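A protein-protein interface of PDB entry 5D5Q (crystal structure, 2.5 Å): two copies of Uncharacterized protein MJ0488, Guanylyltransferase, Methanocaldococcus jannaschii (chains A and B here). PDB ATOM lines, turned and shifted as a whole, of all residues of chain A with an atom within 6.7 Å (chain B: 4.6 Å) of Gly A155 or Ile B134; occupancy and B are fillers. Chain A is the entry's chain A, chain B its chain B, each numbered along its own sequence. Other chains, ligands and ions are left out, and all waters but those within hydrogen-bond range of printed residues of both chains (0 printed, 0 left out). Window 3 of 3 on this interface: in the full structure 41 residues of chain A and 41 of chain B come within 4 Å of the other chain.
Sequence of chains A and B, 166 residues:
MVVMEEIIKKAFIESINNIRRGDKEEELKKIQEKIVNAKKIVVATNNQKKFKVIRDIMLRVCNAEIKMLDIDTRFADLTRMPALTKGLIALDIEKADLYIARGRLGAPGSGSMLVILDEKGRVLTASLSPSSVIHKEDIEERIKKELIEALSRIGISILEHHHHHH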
ATOM      1  N   GLU A  25      -4.771 -14.294 -17.536  1.00  0.00           N
ATOM      2  CA  GLU A  25      -3.806 -13.458 -18.235  1.00  0.00           C
ATOM      3  C   GLU A  25      -3.253 -14.145 -19.483  1.00  0.00           C
ATOM      4  O   GLU A  25      -2.974 -13.487 -20.493  1.00  0.00           O
ATOM      5  CB  GLU A  25      -2.683 -13.063 -17.280  1.00  0.00           C
ATOM      6  CG  GLU A  25      -1.486 -12.343 -17.901  1.00  0.00           C
ATOM      7  CD  GLU A  25      -1.838 -11.259 -18.896  1.00  0.00           C
ATOM      8  OE1 GLU A  25      -2.822 -10.525 -18.705  1.00  0.00           O
ATOM      9  OE2 GLU A  25      -1.087 -11.145 -19.877  1.00  0.00           O
ATOM     10  N   LEU A  28      -5.942 -13.756 -22.296  1.00  0.00           N
ATOM     11  CA  LEU A  28      -5.861 -12.418 -22.855  1.00  0.00           C
ATOM     12  C   LEU A  28      -4.632 -12.211 -23.737  1.00  0.00           C
ATOM     13  O   LEU A  28      -4.737 -11.629 -24.816  1.00  0.00           O
ATOM     14  CB  LEU A  28      -5.852 -11.396 -21.726  1.00  0.00           C
ATOM     15  CG  LEU A  28      -5.834  -9.939 -22.170  1.00  0.00           C
ATOM     16  CD1 LEU A  28      -7.142  -9.539 -22.834  1.00  0.00           C
ATOM     17  CD2 LEU A  28      -5.514  -9.068 -20.982  1.00  0.00           C
ATOM     18  N   LYS A  29      -3.471 -12.678 -23.284  1.00  0.00           N
ATOM     19  CA  LYS A  29      -2.256 -12.498 -24.075  1.00  0.00           C
ATOM     20  C   LYS A  29      -2.310 -13.374 -25.315  1.00  0.00           C
ATOM     21  O   LYS A  29      -1.720 -13.046 -26.346  1.00  0.00           O
ATOM     22  CB  LYS A  29      -0.996 -12.812 -23.266  1.00  0.00           C
ATOM     23  CG  LYS A  29      -0.193 -11.581 -22.877  1.00  0.00           C
ATOM     24  CD  LYS A  29      -1.080 -10.338 -22.782  1.00  0.00           C
ATOM     25  CE  LYS A  29      -0.270  -9.116 -22.365  1.00  0.00           C
ATOM     26  NZ  LYS A  29      -1.118  -7.889 -22.382  1.00  0.00           N
ATOM     27  N   GLN A  32      -4.470 -11.234 -27.682  1.00  0.00           N
ATOM     28  CA  GLN A  32      -3.666 -10.137 -28.210  1.00  0.00           C
ATOM     29  C   GLN A  32      -2.660 -10.609 -29.237  1.00  0.00           C
ATOM     30  O   GLN A  32      -2.555 -10.033 -30.312  1.00  0.00           O
ATOM     31  CB  GLN A  32      -2.909  -9.411 -27.103  1.00  0.00           C
ATOM     32  CG  GLN A  32      -3.761  -8.632 -26.144  1.00  0.00           C
ATOM     33  CD  GLN A  32      -2.930  -7.997 -25.057  1.00  0.00           C
ATOM     34  OE1 GLN A  32      -1.724  -8.220 -24.977  1.00  0.00           O
ATOM     35  NE2 GLN A  32      -3.569  -7.216 -24.202  1.00  0.00           N
ATOM     36  N   ALA A 150     -12.586  -1.640 -28.914  1.00  0.00           N
ATOM     37  CA  ALA A 150     -12.531  -3.092 -29.044  1.00  0.00           C
ATOM     38  C   ALA A 150     -11.106  -3.617 -28.897  1.00  0.00           C
ATOM     39  O   ALA A 150     -10.888  -4.671 -28.302  1.00  0.00           O
ATOM     40  CB  ALA A 150     -13.119  -3.524 -30.381  1.00  0.00           C
ATOM     41  N   LEU A 151     -10.138  -2.881 -29.435  1.00  0.00           N
ATOM     42  CA  LEU A 151      -8.738  -3.270 -29.292  1.00  0.00           C
ATOM     43  C   LEU A 151      -8.198  -2.988 -27.891  1.00  0.00           C
ATOM     44  O   LEU A 151      -7.491  -3.808 -27.310  1.00  0.00           O
ATOM     45  CB  LEU A 151      -7.875  -2.553 -30.333  1.00  0.00           C
ATOM     46  CG  LEU A 151      -8.154  -2.881 -31.801  1.00  0.00           C
ATOM     47  CD1 LEU A 151      -7.353  -1.970 -32.718  1.00  0.00           C
ATOM     48  CD2 LEU A 151      -7.854  -4.342 -32.094  1.00  0.00           C
ATOM     49  N   SER A 152      -8.545  -1.827 -27.347  1.00  0.00           N
ATOM     50  CA  SER A 152      -8.038  -1.403 -26.045  1.00  0.00           C
ATOM     51  C   SER A 152      -8.558  -2.251 -24.887  1.00  0.00           C
ATOM     52  O   SER A 152      -7.820  -2.545 -23.946  1.00  0.00           O
ATOM     53  CB  SER A 152      -8.389   0.065 -25.796  1.00  0.00           C
ATOM     54  OG  SER A 152      -9.658   0.185 -25.178  1.00  0.00           O
ATOM     55  N   ARG A 153      -9.826  -2.646 -24.962  1.00  0.00           N
ATOM     56  CA  ARG A 153     -10.455  -3.407 -23.887  1.00  0.00           C
ATOM     57  C   ARG A 153      -9.800  -4.772 -23.687  1.00  0.00           C
ATOM     58  O   ARG A 153      -9.989  -5.411 -22.654  1.00  0.00           O
ATOM     59  CB  ARG A 153     -11.951  -3.574 -24.149  1.00  0.00           C
ATOM     60  CG  ARG A 153     -12.293  -4.535 -25.263  1.00  0.00           C
ATOM     61  CD  ARG A 153     -13.782  -4.504 -25.548  1.00  0.00           C
ATOM     62  NE  ARG A 153     -14.566  -5.136 -24.490  1.00  0.00           N
ATOM     63  CZ  ARG A 153     -14.732  -6.449 -24.364  1.00  0.00           C
ATOM     64  NH1 ARG A 153     -15.462  -6.935 -23.369  1.00  0.00           N
ATOM     65  NH2 ARG A 153     -14.169  -7.277 -25.233  1.00  0.00           N
ATOM     66  N   ILE A 154      -9.035  -5.222 -24.675  1.00  0.00           N
ATOM     67  CA  ILE A 154      -8.289  -6.463 -24.525  1.00  0.00           C
ATOM     68  C   ILE A 154      -6.793  -6.159 -24.476  1.00  0.00           C
ATOM     69  O   ILE A 154      -5.966  -7.054 -24.627  1.00  0.00           O
ATOM     70  CB  ILE A 154      -8.595  -7.476 -25.655  1.00  0.00           C
ATOM     71  CG1 ILE A 154      -8.508  -6.809 -27.028  1.00  0.00           C
ATOM     72  CG2 ILE A 154      -9.968  -8.101 -25.455  1.00  0.00           C
ATOM     73  CD1 ILE A 154      -8.428  -7.794 -28.175  1.00  0.00           C
ATOM     74  N   GLY A 155      -6.454  -4.891 -24.251  1.00  0.00           N
ATOM     75  CA  GLY A 155      -5.080  -4.515 -23.963  1.00  0.00           C
ATOM     76  C   GLY A 155      -4.203  -4.188 -25.155  1.00  0.00           C
ATOM     77  O   GLY A 155      -2.975  -4.206 -25.061  1.00  0.00           O
ATOM     78  N   ILE A 156      -4.832  -3.886 -26.281  1.00  0.00           N
ATOM     79  CA  ILE A 156      -4.111  -3.580 -27.510  1.00  0.00           C
ATOM     80  C   ILE A 156      -4.083  -2.088 -27.798  1.00  0.00           C
ATOM     81  O   ILE A 156      -5.126  -1.452 -27.936  1.00  0.00           O
ATOM     82  CB  ILE A 156      -4.709  -4.310 -28.707  1.00  0.00           C
ATOM     83  CG1 ILE A 156      -4.471  -5.812 -28.556  1.00  0.00           C
ATOM     84  CG2 ILE A 156      -4.070  -3.820 -29.986  1.00  0.00           C
ATOM     85  CD1 ILE A 156      -4.974  -6.624 -29.711  1.00  0.00           C
ATOM     86  N   SER A 157      -2.880  -1.530 -27.875  1.00  0.00           N
ATOM     87  CA  SER A 157      -2.741  -0.115 -28.178  1.00  0.00           C
ATOM     88  C   SER A 157      -2.536   0.201 -29.652  1.00  0.00           C
ATOM     89  O   SER A 157      -1.680  -0.375 -30.325  1.00  0.00           O
ATOM     90  CB  SER A 157      -1.557   0.455 -27.398  1.00  0.00           C
ATOM     91  OG  SER A 157      -0.860   1.418 -28.175  1.00  0.00           O
ATOM     92  N   SER B 131     -11.248  -7.115 -20.185  1.00  0.00           N
ATOM     93  CA  SER B 131     -10.954  -8.319 -19.420  1.00  0.00           C
ATOM     94  C   SER B 131     -10.698  -7.958 -17.961  1.00  0.00           C
ATOM     95  O   SER B 131     -10.041  -6.958 -17.672  1.00  0.00           O
ATOM     96  CB  SER B 131      -9.751  -9.053 -20.013  1.00  0.00           C
ATOM     97  OG  SER B 131      -9.505 -10.269 -19.331  1.00  0.00           O
ATOM     98  N   SER B 132     -11.226  -8.769 -17.047  1.00  0.00           N
ATOM     99  CA  SER B 132     -11.021  -8.552 -15.619  1.00  0.00           C
ATOM    100  C   SER B 132      -9.540  -8.639 -15.284  1.00  0.00           C
ATOM    101  O   SER B 132      -9.090  -8.153 -14.246  1.00  0.00           O
ATOM    102  CB  SER B 132     -11.806  -9.574 -14.796  1.00  0.00           C
ATOM    103  OG  SER B 132     -11.417 -10.896 -15.130  1.00  0.00           O
ATOM    104  N   VAL B 133      -8.791  -9.268 -16.179  1.00  0.00           N
ATOM    105  CA  VAL B 133      -7.348  -9.329 -16.076  1.00  0.00           C
ATOM    106  C   VAL B 133      -6.775  -7.916 -16.145  1.00  0.00           C
ATOM    107  O   VAL B 133      -5.818  -7.583 -15.441  1.00  0.00           O
ATOM    108  CB  VAL B 133      -6.749 -10.195 -17.191  1.00  0.00           C
ATOM    109  CG1 VAL B 133      -5.256 -10.109 -17.146  1.00  0.00           C
ATOM    110  CG2 VAL B 133      -7.190 -11.637 -17.034  1.00  0.00           C
ATOM    111  N   ILE B 134      -7.385  -7.085 -16.985  1.00  0.00           N
ATOM    112  CA  ILE B 134      -6.918  -5.717 -17.191  1.00  0.00           C
ATOM    113  C   ILE B 134      -7.484  -4.685 -16.214  1.00  0.00           C
ATOM    114  O   ILE B 134      -6.743  -3.868 -15.677  1.00  0.00           O
ATOM    115  CB  ILE B 134      -7.245  -5.224 -18.626  1.00  0.00           C
ATOM    116  CG1 ILE B 134      -6.469  -6.025 -19.668  1.00  0.00           C
ATOM    117  CG2 ILE B 134      -6.889  -3.759 -18.801  1.00  0.00           C
ATOM    118  CD1 ILE B 134      -6.945  -5.786 -21.082  1.00  0.00           C
ATOM    119  N   HIS B 135      -8.786  -4.733 -15.962  1.00  0.00           N
ATOM    120  CA  HIS B 135      -9.412  -3.706 -15.135  1.00  0.00           C
ATOM    121  C   HIS B 135      -9.499  -4.034 -13.657  1.00  0.00           C
ATOM    122  O   HIS B 135     -10.106  -3.270 -12.914  1.00  0.00           O
ATOM    123  CB  HIS B 135     -10.833  -3.398 -15.651  1.00  0.00           C
ATOM    124  CG  HIS B 135     -11.836  -4.465 -15.378  1.00  0.00           C
ATOM    125  ND1 HIS B 135     -12.355  -4.718 -14.110  1.00  0.00           N
ATOM    126  CD2 HIS B 135     -12.462  -5.353 -16.191  1.00  0.00           C
ATOM    127  CE1 HIS B 135     -13.217  -5.697 -14.165  1.00  0.00           C
ATOM    128  NE2 HIS B 135     -13.307  -6.107 -15.434  1.00  0.00           N
ATOM    129  N   LYS B 136      -8.853  -5.127 -13.245  1.00  0.00           N
ATOM    130  CA  LYS B 136      -8.869  -5.667 -11.871  1.00  0.00           C
ATOM    131  C   LYS B 136      -9.819  -5.005 -10.877  1.00  0.00           C
ATOM    132  O   LYS B 136      -9.444  -4.727  -9.744  1.00  0.00           O
ATOM    133  CB  LYS B 136      -7.457  -5.590 -11.283  1.00  0.00           C
ATOM    134  CG  LYS B 136      -6.412  -6.147 -12.216  1.00  0.00           C
ATOM    135  CD  LYS B 136      -5.159  -5.289 -12.208  1.00  0.00           C
ATOM    136  CE  LYS B 136      -4.190  -5.771 -13.280  1.00  0.00           C
ATOM    137  NZ  LYS B 136      -3.328  -4.715 -13.903  1.00  0.00           N
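O of Arg A153 is in hydrogen-bond range of N of Ser B131.
The side-chain amide nitrogen (NE2) of Gln A32 sits close to the backbone carbonyl oxygen (O) of Gly A155, at 3.2 Å. The side-chain amide nitrogen of Gln A32 lies within hydrogen-bond range of the backbone carbonyl oxygen of Ile A154, 2.4 Å away. The backbone NH (N) of Val B133 sits close to the side-chain hydroxyl (OG) of Ser B131 (3.4 Å).
Glu A25 touches Val B133 (OE1 to CG1, 2.9 Å). Leu A28 touches Ser B131. Val B133 touches Leu A28. CG1 of Ile B134 touches CD2 of Leu A28, 3.4 Å away. Arg A153 touches Ile B134 (O to CD1, 3.4 Å). CD1 of Ile B134 touches C of Ile A154, at 3.4 Å. Gly A155 touches Ile B134 (N to CD1, 3.3 Å).
Of chain B, only Ile B134 (3.3 Å) comes within 4 Å of Gly A155. Printed residues of chain A within 4 Å of Ile B134: Leu A28 (3.4 Å), Arg A153 (3.4 Å), Ile A154 (3.4 Å) and Gly A155 (3.3 Å). Printed residues of chain B within 4 Å of Arg A153: Ser B131 and Ile B134. Of the printed residues of chain A, Val B133 touches Glu A25 and Leu A28. Leu A151 touches none of the printed residues of chain B. Ile A156 touches none of the printed residues of chain B. The nearest printed residue of chain B that does not touch Gly A155 is Ser B131 (6.7 Å). The nearest printed residue of chain B that does not touch Glu A25 is Ile B134 (5.9 Å).
Of the 12 printed residues of chain A, 5 touch a printed residue of chain B. Hydrophobic or aromatic side chains of chain A within 4 Å of the printed part of chain B: Leu A28. Hydrophobic or aromatic side chains of chain B within 4 Å of the printed part of chain A: Val B133 and Ile B134. Among the printed residues, no Asp or Glu carboxylate lies within 4 Å of a Lys or Arg side-chain nitrogen of the other chain.
No position is printed for both chains. Of the 8 pairs that touch across the chains among the printed residues, none has its exchanged pair printed and touching as well.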
